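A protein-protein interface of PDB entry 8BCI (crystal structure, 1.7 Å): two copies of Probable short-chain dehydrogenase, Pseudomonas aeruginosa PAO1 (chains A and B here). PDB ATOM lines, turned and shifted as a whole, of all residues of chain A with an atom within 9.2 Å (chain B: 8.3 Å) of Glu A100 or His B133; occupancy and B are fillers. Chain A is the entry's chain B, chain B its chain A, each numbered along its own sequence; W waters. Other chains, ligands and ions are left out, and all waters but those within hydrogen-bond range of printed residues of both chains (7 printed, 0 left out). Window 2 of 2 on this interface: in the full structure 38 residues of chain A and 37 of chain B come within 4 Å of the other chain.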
ATOM      1  N   THR A  97      20.012  -9.777  32.308  1.00  0.00           N
ATOM      2  CA  THR A  97      20.109 -11.019  31.558  1.00  0.00           C
ATOM      3  C   THR A  97      18.701 -11.503  31.242  1.00  0.00           C
ATOM      4  O   THR A  97      17.747 -11.167  31.951  1.00  0.00           O
ATOM      5  CB  THR A  97      20.820 -12.094  32.408  1.00  0.00           C
ATOM      6  OG1 THR A  97      21.050 -13.272  31.645  1.00  0.00           O
ATOM      7  CG2 THR A  97      19.944 -12.459  33.594  1.00  0.00           C
ATOM      8  N   ARG A  98      18.578 -12.281  30.177  1.00  0.00           N
ATOM      9  CA  ARG A  98      17.369 -13.058  29.941  1.00  0.00           C
ATOM     10  C   ARG A  98      17.509 -14.414  30.625  1.00  0.00           C
ATOM     11  O   ARG A  98      18.614 -14.880  30.908  1.00  0.00           O
ATOM     12  CB  ARG A  98      17.129 -13.215  28.442  1.00  0.00           C
ATOM     13  CG  ARG A  98      16.902 -11.834  27.770  1.00  0.00           C
ATOM     14  CD  ARG A  98      16.716 -11.919  26.272  1.00  0.00           C
ATOM     15  NE  ARG A  98      15.430 -12.483  25.894  1.00  0.00           N
ATOM     16  CZ  ARG A  98      14.295 -11.804  25.854  1.00  0.00           C
ATOM     17  NH1 ARG A  98      14.235 -10.548  26.235  1.00  0.00           N
ATOM     18  NH2 ARG A  98      13.202 -12.395  25.383  1.00  0.00           N
ATOM     19  N   LEU A  99      16.365 -15.046  30.903  1.00  0.00           N
ATOM     20  CA  LEU A  99      16.397 -16.286  31.670  1.00  0.00           C
ATOM     21  C   LEU A  99      17.150 -17.371  30.935  1.00  0.00           C
ATOM     22  O   LEU A  99      17.794 -18.221  31.572  1.00  0.00           O
ATOM     23  CB  LEU A  99      14.971 -16.739  32.021  1.00  0.00           C
ATOM     24  CG  LEU A  99      14.802 -18.021  32.809  1.00  0.00           C
ATOM     25  CD1 LEU A  99      13.618 -17.958  33.780  1.00  0.00           C
ATOM     26  CD2 LEU A  99      14.604 -19.207  31.869  1.00  0.00           C
ATOM     27  N   GLU A 100      17.134 -17.348  29.601  1.00  0.00           N
ATOM     28  CA  GLU A 100      17.844 -18.408  28.884  1.00  0.00           C
ATOM     29  C   GLU A 100      19.352 -18.341  29.081  1.00  0.00           C
ATOM     30  O   GLU A 100      20.055 -19.306  28.727  1.00  0.00           O
ATOM     31  CB  GLU A 100      17.488 -18.364  27.416  1.00  0.00           C
ATOM     32  CG  GLU A 100      18.051 -17.255  26.637  1.00  0.00           C
ATOM     33  CD  GLU A 100      17.879 -17.536  25.136  1.00  0.00           C
ATOM     34  OE1 GLU A 100      18.413 -18.533  24.610  1.00  0.00           O
ATOM     35  OE2 GLU A 100      17.188 -16.756  24.494  1.00  0.00           O
ATOM     36  N   ASN A 101      19.857 -17.260  29.671  1.00  0.00           N
ATOM     37  CA  ASN A 101      21.271 -17.127  29.974  1.00  0.00           C
ATOM     38  C   ASN A 101      21.603 -17.189  31.455  1.00  0.00           C
ATOM     39  O   ASN A 101      22.760 -16.948  31.822  1.00  0.00           O
ATOM     40  CB  ASN A 101      21.787 -15.824  29.373  1.00  0.00           C
ATOM     41  CG  ASN A 101      21.716 -15.840  27.855  1.00  0.00           C
ATOM     42  OD1 ASN A 101      22.062 -16.848  27.240  1.00  0.00           O
ATOM     43  ND2 ASN A 101      21.204 -14.782  27.265  1.00  0.00           N
ATOM     44  N   ILE A 102      20.647 -17.533  32.299  1.00  0.00           N
ATOM     45  CA  ILE A 102      20.877 -17.666  33.733  1.00  0.00           C
ATOM     46  C   ILE A 102      21.303 -19.101  34.013  1.00  0.00           C
ATOM     47  O   ILE A 102      20.549 -20.041  33.740  1.00  0.00           O
ATOM     48  CB  ILE A 102      19.622 -17.306  34.530  1.00  0.00           C
ATOM     49  CG1 ILE A 102      19.312 -15.810  34.357  1.00  0.00           C
ATOM     50  CG2 ILE A 102      19.826 -17.613  36.005  1.00  0.00           C
ATOM     51  CD1 ILE A 102      18.044 -15.402  35.067  1.00  0.00           C
ATOM     52  N   ASP A 103      22.499 -19.278  34.559  1.00  0.00           N
ATOM     53  CA  ASP A 103      22.952 -20.638  34.829  1.00  0.00           C
ATOM     54  C   ASP A 103      22.763 -21.000  36.307  1.00  0.00           C
ATOM     55  O   ASP A 103      22.341 -20.197  37.139  1.00  0.00           O
ATOM     56  CB  ASP A 103      24.404 -20.849  34.362  1.00  0.00           C
ATOM     57  CG  ASP A 103      25.419 -20.002  35.077  1.00  0.00           C
ATOM     58  OD1 ASP A 103      25.157 -19.377  36.138  1.00  0.00           O
ATOM     59  OD2 ASP A 103      26.565 -19.958  34.569  1.00  0.00           O
ATOM     60  N   ALA A 104      23.039 -22.265  36.625  1.00  0.00           N
ATOM     61  CA  ALA A 104      22.758 -22.750  37.972  1.00  0.00           C
ATOM     62  C   ALA A 104      23.598 -22.004  39.012  1.00  0.00           C
ATOM     63  O   ALA A 104      23.133 -21.721  40.117  1.00  0.00           O
ATOM     64  CB  ALA A 104      22.989 -24.259  38.025  1.00  0.00           C
ATOM     65  N   ASN A 154      13.552  -9.505  31.038  1.00  0.00           N
ATOM     66  CA  ASN A 154      14.712  -9.015  30.291  1.00  0.00           C
ATOM     67  C   ASN A 154      15.782  -8.412  31.191  1.00  0.00           C
ATOM     68  O   ASN A 154      16.680  -7.712  30.698  1.00  0.00           O
ATOM     69  CB  ASN A 154      14.285  -7.990  29.233  1.00  0.00           C
ATOM     70  CG  ASN A 154      15.335  -7.779  28.165  1.00  0.00           C
ATOM     71  OD1 ASN A 154      15.978  -8.719  27.725  1.00  0.00           O
ATOM     72  ND2 ASN A 154      15.495  -6.523  27.725  1.00  0.00           N
ATOM     73  N   ILE A 157      14.890 -12.204  36.085  1.00  0.00           N
ATOM     74  CA  ILE A 157      13.779 -13.009  36.601  1.00  0.00           C
ATOM     75  C   ILE A 157      14.197 -13.816  37.813  1.00  0.00           C
ATOM     76  O   ILE A 157      13.364 -14.094  38.688  1.00  0.00           O
ATOM     77  CB  ILE A 157      13.231 -13.910  35.491  1.00  0.00           C
ATOM     78  CG1 ILE A 157      12.626 -13.045  34.377  1.00  0.00           C
ATOM     79  CG2 ILE A 157      12.197 -14.819  36.010  1.00  0.00           C
ATOM     80  CD1 ILE A 157      12.283 -13.838  33.113  1.00  0.00           C
ATOM     81  N   ASP A 158      15.492 -14.166  37.918  1.00  0.00           N
ATOM     82  CA  ASP A 158      15.971 -14.873  39.103  1.00  0.00           C
ATOM     83  C   ASP A 158      15.776 -14.040  40.367  1.00  0.00           C
ATOM     84  O   ASP A 158      15.338 -14.563  41.394  1.00  0.00           O
ATOM     85  CB  ASP A 158      17.436 -15.275  38.929  1.00  0.00           C
ATOM     86  CG  ASP A 158      18.372 -14.122  38.588  1.00  0.00           C
ATOM     87  OD1 ASP A 158      18.017 -13.144  37.914  1.00  0.00           O
ATOM     88  OD2 ASP A 158      19.547 -14.201  38.959  1.00  0.00           O
ATOM     89  N   GLU B  66      22.489 -29.163  36.685  1.00  0.00           N
ATOM     90  CA  GLU B  66      22.595 -28.611  35.343  1.00  0.00           C
ATOM     91  C   GLU B  66      23.049 -29.649  34.323  1.00  0.00           C
ATOM     92  O   GLU B  66      22.548 -29.675  33.187  1.00  0.00           O
ATOM     93  CB  GLU B  66      23.569 -27.446  35.400  1.00  0.00           C
ATOM     94  CG  GLU B  66      23.457 -26.481  34.310  1.00  0.00           C
ATOM     95  CD  GLU B  66      24.117 -25.187  34.683  1.00  0.00           C
ATOM     96  OE1 GLU B  66      25.247 -25.227  35.255  1.00  0.00           O
ATOM     97  OE2 GLU B  66      23.484 -24.165  34.417  1.00  0.00           O
ATOM     98  N   PHE B 119      13.687 -23.298  36.759  1.00  0.00           N
ATOM     99  CA  PHE B 119      14.462 -22.347  35.967  1.00  0.00           C
ATOM    100  C   PHE B 119      15.274 -23.054  34.888  1.00  0.00           C
ATOM    101  O   PHE B 119      15.287 -22.658  33.725  1.00  0.00           O
ATOM    102  CB  PHE B 119      15.414 -21.522  36.847  1.00  0.00           C
ATOM    103  CG  PHE B 119      14.817 -20.235  37.384  1.00  0.00           C
ATOM    104  CD1 PHE B 119      13.957 -20.236  38.443  1.00  0.00           C
ATOM    105  CD2 PHE B 119      15.169 -19.018  36.806  1.00  0.00           C
ATOM    106  CE1 PHE B 119      13.431 -19.089  38.939  1.00  0.00           C
ATOM    107  CE2 PHE B 119      14.655 -17.840  37.300  1.00  0.00           C
ATOM    108  CZ  PHE B 119      13.766 -17.875  38.336  1.00  0.00           C
ATOM    109  N   LEU B 120      16.014 -24.102  35.268  1.00  0.00           N
ATOM    110  CA  LEU B 120      16.920 -24.722  34.319  1.00  0.00           C
ATOM    111  C   LEU B 120      16.157 -25.385  33.182  1.00  0.00           C
ATOM    112  O   LEU B 120      16.574 -25.313  32.023  1.00  0.00           O
ATOM    113  CB  LEU B 120      17.808 -25.749  35.018  1.00  0.00           C
ATOM    114  CG  LEU B 120      18.777 -25.153  36.040  1.00  0.00           C
ATOM    115  CD1 LEU B 120      19.561 -26.294  36.682  1.00  0.00           C
ATOM    116  CD2 LEU B 120      19.722 -24.188  35.379  1.00  0.00           C
ATOM    117  N   ALA B 122      13.079 -24.450  32.212  1.00  0.00           N
ATOM    118  CA  ALA B 122      12.510 -23.359  31.413  1.00  0.00           C
ATOM    119  C   ALA B 122      13.556 -22.796  30.455  1.00  0.00           C
ATOM    120  O   ALA B 122      13.247 -22.466  29.294  1.00  0.00           O
ATOM    121  CB  ALA B 122      11.939 -22.258  32.322  1.00  0.00           C
ATOM    122  N   ARG B 123      14.809 -22.698  30.912  1.00  0.00           N
ATOM    123  CA  ARG B 123      15.885 -22.173  30.073  1.00  0.00           C
ATOM    124  C   ARG B 123      16.127 -23.059  28.854  1.00  0.00           C
ATOM    125  O   ARG B 123      16.235 -22.578  27.725  1.00  0.00           O
ATOM    126  CB  ARG B 123      17.154 -22.042  30.921  1.00  0.00           C
ATOM    127  CG  ARG B 123      18.475 -21.908  30.163  1.00  0.00           C
ATOM    128  CD  ARG B 123      19.523 -21.436  31.150  1.00  0.00           C
ATOM    129  NE  ARG B 123      20.883 -21.296  30.627  1.00  0.00           N
ATOM    130  CZ  ARG B 123      21.934 -21.956  31.092  1.00  0.00           C
ATOM    131  NH1 ARG B 123      21.791 -22.994  31.906  1.00  0.00           N
ATOM    132  NH2 ARG B 123      23.159 -21.537  30.772  1.00  0.00           N
ATOM    133  N   GLU B 124      16.210 -24.368  29.064  1.00  0.00           N
ATOM    134  CA  GLU B 124      16.363 -25.274  27.938  1.00  0.00           C
ATOM    135  C   GLU B 124      15.151 -25.281  27.023  1.00  0.00           C
ATOM    136  O   GLU B 124      15.315 -25.429  25.800  1.00  0.00           O
ATOM    137  CB  GLU B 124      16.656 -26.699  28.422  1.00  0.00           C
ATOM    138  CG  GLU B 124      17.983 -26.823  29.164  1.00  0.00           C
ATOM    139  CD  GLU B 124      19.162 -26.300  28.353  1.00  0.00           C
ATOM    140  OE1 GLU B 124      19.285 -26.687  27.161  1.00  0.00           O
ATOM    141  OE2 GLU B 124      19.924 -25.472  28.893  1.00  0.00           O
ATOM    142  N   ALA B 125      13.951 -25.121  27.587  1.00  0.00           N
ATOM    143  CA  ALA B 125      12.740 -25.021  26.772  1.00  0.00           C
ATOM    144  C   ALA B 125      12.745 -23.760  25.910  1.00  0.00           C
ATOM    145  O   ALA B 125      12.433 -23.820  24.718  1.00  0.00           O
ATOM    146  CB  ALA B 125      11.504 -25.090  27.682  1.00  0.00           C
ATOM    147  N   VAL B 126      13.162 -22.620  26.470  1.00  0.00           N
ATOM    148  CA  VAL B 126      13.201 -21.385  25.673  1.00  0.00           C
ATOM    149  C   VAL B 126      14.142 -21.557  24.496  1.00  0.00           C
ATOM    150  O   VAL B 126      13.886 -21.069  23.380  1.00  0.00           O
ATOM    151  CB  VAL B 126      13.602 -20.182  26.562  1.00  0.00           C
ATOM    152  CG1 VAL B 126      13.991 -18.983  25.716  1.00  0.00           C
ATOM    153  CG2 VAL B 126      12.477 -19.830  27.516  1.00  0.00           C
ATOM    154  N   LYS B 127      15.254 -22.255  24.721  1.00  0.00           N
ATOM    155  CA  LYS B 127      16.248 -22.421  23.669  1.00  0.00           C
ATOM    156  C   LYS B 127      15.696 -23.186  22.476  1.00  0.00           C
ATOM    157  O   LYS B 127      16.175 -22.991  21.349  1.00  0.00           O
ATOM    158  CB  LYS B 127      17.476 -23.105  24.234  1.00  0.00           C
ATOM    159  CG  LYS B 127      18.324 -22.175  25.111  1.00  0.00           C
ATOM    160  CD  LYS B 127      19.492 -22.931  25.722  1.00  0.00           C
ATOM    161  CE  LYS B 127      20.345 -22.085  26.673  1.00  0.00           C
ATOM    162  NZ  LYS B 127      20.815 -20.804  26.070  1.00  0.00           N
ATOM    163  N   ARG B 128      14.707 -24.050  22.701  1.00  0.00           N
ATOM    164  CA  ARG B 128      14.105 -24.864  21.655  1.00  0.00           C
ATOM    165  C   ARG B 128      12.794 -24.315  21.126  1.00  0.00           C
ATOM    166  O   ARG B 128      12.565 -24.414  19.920  1.00  0.00           O
ATOM    167  CB  ARG B 128      13.880 -26.283  22.166  1.00  0.00           C
ATOM    168  CG  ARG B 128      15.247 -26.981  22.321  1.00  0.00           C
ATOM    169  CD  ARG B 128      15.200 -28.077  23.312  1.00  0.00           C
ATOM    170  NE  ARG B 128      16.498 -28.742  23.381  1.00  0.00           N
ATOM    171  CZ  ARG B 128      17.509 -28.394  24.169  1.00  0.00           C
ATOM    172  NH1 ARG B 128      17.432 -27.353  24.999  1.00  0.00           N
ATOM    173  NH2 ARG B 128      18.647 -29.086  24.095  1.00  0.00           N
ATOM    174  N   LEU B 129      11.928 -23.777  21.997  1.00  0.00           N
ATOM    175  CA  LEU B 129      10.633 -23.264  21.559  1.00  0.00           C
ATOM    176  C   LEU B 129      10.728 -21.907  20.860  1.00  0.00           C
ATOM    177  O   LEU B 129       9.831 -21.562  20.079  1.00  0.00           O
ATOM    178  CB  LEU B 129       9.706 -23.115  22.746  1.00  0.00           C
ATOM    179  CG  LEU B 129       9.004 -24.334  23.321  1.00  0.00           C
ATOM    180  CD1 LEU B 129       9.910 -25.505  23.516  1.00  0.00           C
ATOM    181  CD2 LEU B 129       8.284 -23.924  24.621  1.00  0.00           C
ATOM    182  N   SER B 130      11.699 -21.077  21.231  1.00  0.00           N
ATOM    183  CA  SER B 130      11.696 -19.674  20.827  1.00  0.00           C
ATOM    184  C   SER B 130      11.756 -19.538  19.321  1.00  0.00           C
ATOM    185  O   SER B 130      12.628 -20.118  18.693  1.00  0.00           O
ATOM    186  CB  SER B 130      12.888 -18.942  21.416  1.00  0.00           C
ATOM    187  OG  SER B 130      13.027 -17.664  20.833  1.00  0.00           O
ATOM    188  N   THR B 131      10.912 -18.668  18.763  1.00  0.00           N
ATOM    189  CA  THR B 131      11.031 -18.358  17.340  1.00  0.00           C
ATOM    190  C   THR B 131      12.358 -17.698  16.980  1.00  0.00           C
ATOM    191  O   THR B 131      12.712 -17.660  15.793  1.00  0.00           O
ATOM    192  CB  THR B 131       9.882 -17.448  16.889  1.00  0.00           C
ATOM    193  OG1 THR B 131       9.926 -16.217  17.621  1.00  0.00           O
ATOM    194  CG2 THR B 131       8.536 -18.098  17.114  1.00  0.00           C
ATOM    195  N   ARG B 132      13.080 -17.152  17.961  1.00  0.00           N
ATOM    196  CA  ARG B 132      14.407 -16.606  17.715  1.00  0.00           C
ATOM    197  C   ARG B 132      15.455 -17.692  17.502  1.00  0.00           C
ATOM    198  O   ARG B 132      16.557 -17.385  17.031  1.00  0.00           O
ATOM    199  CB  ARG B 132      14.869 -15.728  18.877  1.00  0.00           C
ATOM    200  CG  ARG B 132      14.133 -14.402  19.043  1.00  0.00           C
ATOM    201  CD  ARG B 132      14.828 -13.508  20.071  1.00  0.00           C
ATOM    202  NE  ARG B 132      15.584 -14.257  21.070  1.00  0.00           N
ATOM    203  CZ  ARG B 132      16.423 -13.714  21.944  1.00  0.00           C
ATOM    204  NH1 ARG B 132      16.610 -12.406  22.005  1.00  0.00           N
ATOM    205  NH2 ARG B 132      17.093 -14.505  22.776  1.00  0.00           N
ATOM    206  N   HIS B 133      15.145 -18.944  17.855  1.00  0.00           N
ATOM    207  CA  HIS B 133      16.084 -20.052  17.763  1.00  0.00           C
ATOM    208  C   HIS B 133      15.538 -21.163  16.870  1.00  0.00           C
ATOM    209  O   HIS B 133      15.883 -22.334  17.038  1.00  0.00           O
ATOM    210  CB  HIS B 133      16.438 -20.592  19.151  1.00  0.00           C
ATOM    211  CG  HIS B 133      16.936 -19.548  20.100  1.00  0.00           C
ATOM    212  ND1 HIS B 133      17.897 -18.622  19.752  1.00  0.00           N
ATOM    213  CD2 HIS B 133      16.607 -19.284  21.386  1.00  0.00           C
ATOM    214  CE1 HIS B 133      18.130 -17.824  20.780  1.00  0.00           C
ATOM    215  NE2 HIS B 133      17.368 -18.211  21.790  1.00  0.00           N
ATOM    216  N   GLY B 134      14.679 -20.818  15.917  1.00  0.00           N
ATOM    217  CA  GLY B 134      14.151 -21.789  14.989  1.00  0.00           C
ATOM    218  C   GLY B 134      13.021 -22.644  15.491  1.00  0.00           C
ATOM    219  O   GLY B 134      12.691 -23.656  14.877  1.00  0.00           O
ATOM    220  N   GLY B 135      12.400 -22.309  16.614  1.00  0.00           N
ATOM    221  CA  GLY B 135      11.210 -23.000  17.021  1.00  0.00           C
ATOM    222  C   GLY B 135       9.976 -22.303  16.488  1.00  0.00           C
ATOM    223  O   GLY B 135      10.035 -21.234  15.886  1.00  0.00           O
ATOM    224  N   ARG B 136       8.838 -22.931  16.738  1.00  0.00           N
ATOM    225  CA  ARG B 136       7.556 -22.366  16.359  1.00  0.00           C
ATOM    226  C   ARG B 136       6.769 -21.882  17.568  1.00  0.00           C
ATOM    227  O   ARG B 136       5.552 -21.726  17.481  1.00  0.00           O
ATOM    228  CB  ARG B 136       6.732 -23.386  15.584  1.00  0.00           C
ATOM    229  CG  ARG B 136       6.371 -24.664  16.338  1.00  0.00           C
ATOM    230  CD  ARG B 136       5.418 -25.501  15.494  1.00  0.00           C
ATOM    231  NE  ARG B 136       4.680 -26.502  16.251  1.00  0.00           N
ATOM    232  CZ  ARG B 136       3.613 -27.145  15.791  1.00  0.00           C
ATOM    233  NH1 ARG B 136       3.165 -26.945  14.561  1.00  0.00           N
ATOM    234  NH2 ARG B 136       2.979 -28.004  16.584  1.00  0.00           N
ATOM    235  N   GLY B 137       7.446 -21.638  18.684  1.00  0.00           N
ATOM    236  CA  GLY B 137       6.742 -21.304  19.912  1.00  0.00           C
ATOM    237  C   GLY B 137       6.251 -22.532  20.651  1.00  0.00           C
ATOM    238  O   GLY B 137       6.554 -23.671  20.307  1.00  0.00           O
ATOM    239  N   LEU B 173       8.820 -14.477  33.261  1.00  0.00           N
ATOM    240  CA  LEU B 173       9.132 -15.176  32.013  1.00  0.00           C
ATOM    241  C   LEU B 173       8.031 -14.983  30.974  1.00  0.00           C
ATOM    242  O   LEU B 173       8.323 -14.776  29.782  1.00  0.00           O
ATOM    243  CB  LEU B 173       9.391 -16.670  32.289  1.00  0.00           C
ATOM    244  CG  LEU B 173       9.938 -17.455  31.094  1.00  0.00           C
ATOM    245  CD1 LEU B 173      11.205 -16.839  30.526  1.00  0.00           C
ATOM    246  CD2 LEU B 173      10.181 -18.900  31.431  1.00  0.00           C
ATOM    247  N   GLU B 176       8.810 -11.771  29.390  1.00  0.00           N
ATOM    248  CA  GLU B 176      10.081 -11.805  28.674  1.00  0.00           C
ATOM    249  C   GLU B 176       9.990 -12.489  27.325  1.00  0.00           C
ATOM    250  O   GLU B 176      10.573 -11.989  26.350  1.00  0.00           O
ATOM    251  CB  GLU B 176      11.134 -12.489  29.563  1.00  0.00           C
ATOM    252  CG  GLU B 176      12.525 -12.453  28.998  1.00  0.00           C
ATOM    253  CD  GLU B 176      13.587 -12.915  29.984  1.00  0.00           C
ATOM    254  OE1 GLU B 176      13.944 -12.135  30.897  1.00  0.00           O
ATOM    255  OE2 GLU B 176      14.036 -14.070  29.830  1.00  0.00           O
ATOM    256  N   VAL B 177       9.324 -13.648  27.237  1.00  0.00           N
ATOM    257  CA  VAL B 177       9.384 -14.443  26.024  1.00  0.00           C
ATOM    258  C   VAL B 177       8.078 -14.426  25.238  1.00  0.00           C
ATOM    259  O   VAL B 177       7.939 -15.186  24.270  1.00  0.00           O
ATOM    260  CB  VAL B 177       9.828 -15.896  26.310  1.00  0.00           C
ATOM    261  CG1 VAL B 177      11.235 -15.885  26.882  1.00  0.00           C
ATOM    262  CG2 VAL B 177       8.861 -16.622  27.216  1.00  0.00           C
ATOM    263  N   GLU B 180       8.636 -14.120  21.571  1.00  0.00           N
ATOM    264  CA  GLU B 180       9.272 -15.288  20.979  1.00  0.00           C
ATOM    265  C   GLU B 180       8.310 -16.455  20.826  1.00  0.00           C
ATOM    266  O   GLU B 180       8.750 -17.599  20.635  1.00  0.00           O
ATOM    267  CB  GLU B 180      10.439 -15.744  21.856  1.00  0.00           C
ATOM    268  CG  GLU B 180      11.502 -14.732  21.941  1.00  0.00           C
ATOM    269  CD  GLU B 180      12.562 -15.092  22.946  1.00  0.00           C
ATOM    270  OE1 GLU B 180      13.317 -16.049  22.692  1.00  0.00           O
ATOM    271  OE2 GLU B 180      12.656 -14.365  23.948  1.00  0.00           O
ATOM    272  N   ILE B 182       6.235 -17.880  23.068  1.00  0.00           N
ATOM    273  CA  ILE B 182       6.189 -18.803  24.199  1.00  0.00           C
ATOM    274  C   ILE B 182       5.252 -18.229  25.260  1.00  0.00           C
ATOM    275  O   ILE B 182       5.511 -17.138  25.783  1.00  0.00           O
ATOM    276  CB  ILE B 182       7.585 -19.023  24.801  1.00  0.00           C
ATOM    277  CG1 ILE B 182       8.546 -19.607  23.759  1.00  0.00           C
ATOM    278  CG2 ILE B 182       7.503 -19.990  25.972  1.00  0.00           C
ATOM    279  CD1 ILE B 182       9.991 -19.646  24.223  1.00  0.00           C
HETATM  280  O   HOH W   1      11.109  -9.329  25.271  1.00  0.00           O
HETATM  281  O   HOH W   2      14.773 -16.160  28.148  1.00  0.00           O
HETATM  282  O   HOH W   3      23.146 -19.789  28.367  1.00  0.00           O
HETATM  283  O   HOH W   4      15.623 -12.350  33.218  1.00  0.00           O
HETATM  284  O   HOH W   5      24.917 -18.696  30.446  1.00  0.00           O
HETATM  285  O   HOH W   6      17.699 -20.403  34.341  1.00  0.00           O
HETATM  286  O   HOH W   7      26.351 -23.141  36.569  1.00  0.00           O
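The side-chain carboxylate (OE2) of Glu B66 lies within salt-bridge range of the guanidinium group (NH1) of Arg B123 (3.2 Å).
The backbone NH (N) of Thr B131 is in hydrogen-bond range of the backbone carbonyl oxygen (O) of Glu B180, 3.1 Å away.
NH1 of Arg A98 is in hydrogen-bond range of OD1 of Asn A154, at 2.9 Å.
OG of Ser B130 is in hydrogen-bond range of OE1 of Glu B180 (2.5 Å).
The guanidinium group of Arg B132 is in salt-bridge range of the side-chain carboxylate of Glu B180.
The side-chain hydroxyl of Ser B130 lies within hydrogen-bond range of the backbone NH of Arg B132 (2.9 Å).
Of the 24 printed residues of chain B, 11 touch a printed residue of chain A.
Printed residues of chain B that touch a printed residue of chain A: Glu B66, Phe B119, Ala B122, Arg B123, Val B126, Lys B127, Arg B132, His B133, Leu B173, Glu B176 and Glu B180.
Of the 11 printed residues of chain A, 9 touch a printed residue of chain B.
Hydrophobic or aromatic side chains of chain A that line the printed part of chain B: Leu A99, Ala A104 and Ile A157.
Printed residues of chain B within 4 Å of Leu A99: Phe B119, Ala B122, Arg B123 and Glu B176.
Of the printed residues of chain B, Glu A100 touches Arg B123 (2.9 Å), Val B126 (3.9 Å), Lys B127 (3.1 Å), Arg B132 (2.8 Å) and His B133 (3.0 Å).
Of the printed residues of chain B, Ile A102 touches Arg B123 (3.1 Å).
Of the printed residues of chain A, Val B126 touches Glu A100 (3.9 Å).
His B133 touches just one residue of chain A: Glu A100.
Gly B134 touches none of the printed residues of chain A.
Printed residues of chain A within 4 Å of Glu B180: Arg A98.
Water W7 lies within hydrogen-bond range of OE1 of Glu B66 (2.7 Å) and N of Ala A104 (3.4 Å).
Water W4 lies within hydrogen-bond range of the backbone carbonyl oxygen of Thr A97 (2.7 Å), the side-chain carboxylate of Glu B176 (2.9 Å) and the backbone NH of Ile A157 (3.0 Å).
Water W2 lies within hydrogen-bond range of OE2 of Glu B176 (2.8 Å), N of Glu A100 (3.0 Å) and N of Leu A99 (3.4 Å).
Water W6 lies within hydrogen-bond range of O of Ile A102 and O of Phe B119.
Water W3 lies within hydrogen-bond range of the guanidinium group of Arg B123 (3.0 Å), the backbone carbonyl oxygen of Glu A100 (3.1 Å), the side-chain amide oxygen of Asn A101 (3.3 Å) and the side-chain amino group of Lys B127 (3.4 Å).
Water W5 lies within hydrogen-bond range of O of Asn A101 (3.1 Å) and NH2 of Arg B123 (3.4 Å).
No position is printed for both chains.
Of the 20 pairs that touch across the chains among the printed residues, none has its exchanged pair printed and touching as well.
Leu A99 touches Phe B119 (CD1 to CD2, 3.6 Å).
C of Ala B122 touches CD2 of Leu A99, at 3.997 Å.
Leu A99 touches Arg B123 (CD2 to N, 3.6 Å).
CG1 of Val B126 touches CB of Glu A100, at 3.9 Å.
Asp A103 touches Glu B66 (CB to OE2, 3.4 Å).
Asp A103 touches Arg B123 (CB to NH2, 3.9 Å).
CZ of Phe B119 touches O of Ile A157 (3.8 Å).
CD1 of Ile A157 touches N of Leu B173 (3.5 Å).
Glu B176 touches Ile A157.
Asp A158 touches Phe B119.
The backbone carbonyl oxygen (O) of Ile A102 lies close to the guanidinium group (NE) of Arg B123, at 3.4 Å.
The side-chain carboxylate of Glu B66 is in hydrogen-bond range of the backbone NH of Ala A104 (2.9 Å).
The side-chain carboxylate (OE1) of Glu A100 sits at hydrogen-bond distance from a ring nitrogen (NE2) of His B133, at 3.0 Å.
NH2 of Arg B132 lies within salt-bridge range of OE2 of Glu A100 (2.8 Å).
The side-chain carboxylate (OE1) of Glu B176 lies within hydrogen-bond range of the backbone NH (N) of Asn A154.
The guanidinium group (NE) of Arg B123 is in hydrogen-bond range of the backbone carbonyl oxygen (O) of Glu A100 (2.9 Å).
The side-chain carboxylate (OE2) of Glu B180 is in salt-bridge range of the guanidinium group (NH2) of Arg A98.
The backbone NH of Leu A99 lies within hydrogen-bond range of the side-chain carboxylate of Glu B176 (2.7 Å).
NZ of Lys B127 lies within salt-bridge range of OE1 of Glu A100 (3.6 Å).
O of Glu B176 lies within hydrogen-bond range of NH2 of Arg A98 (2.8 Å).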
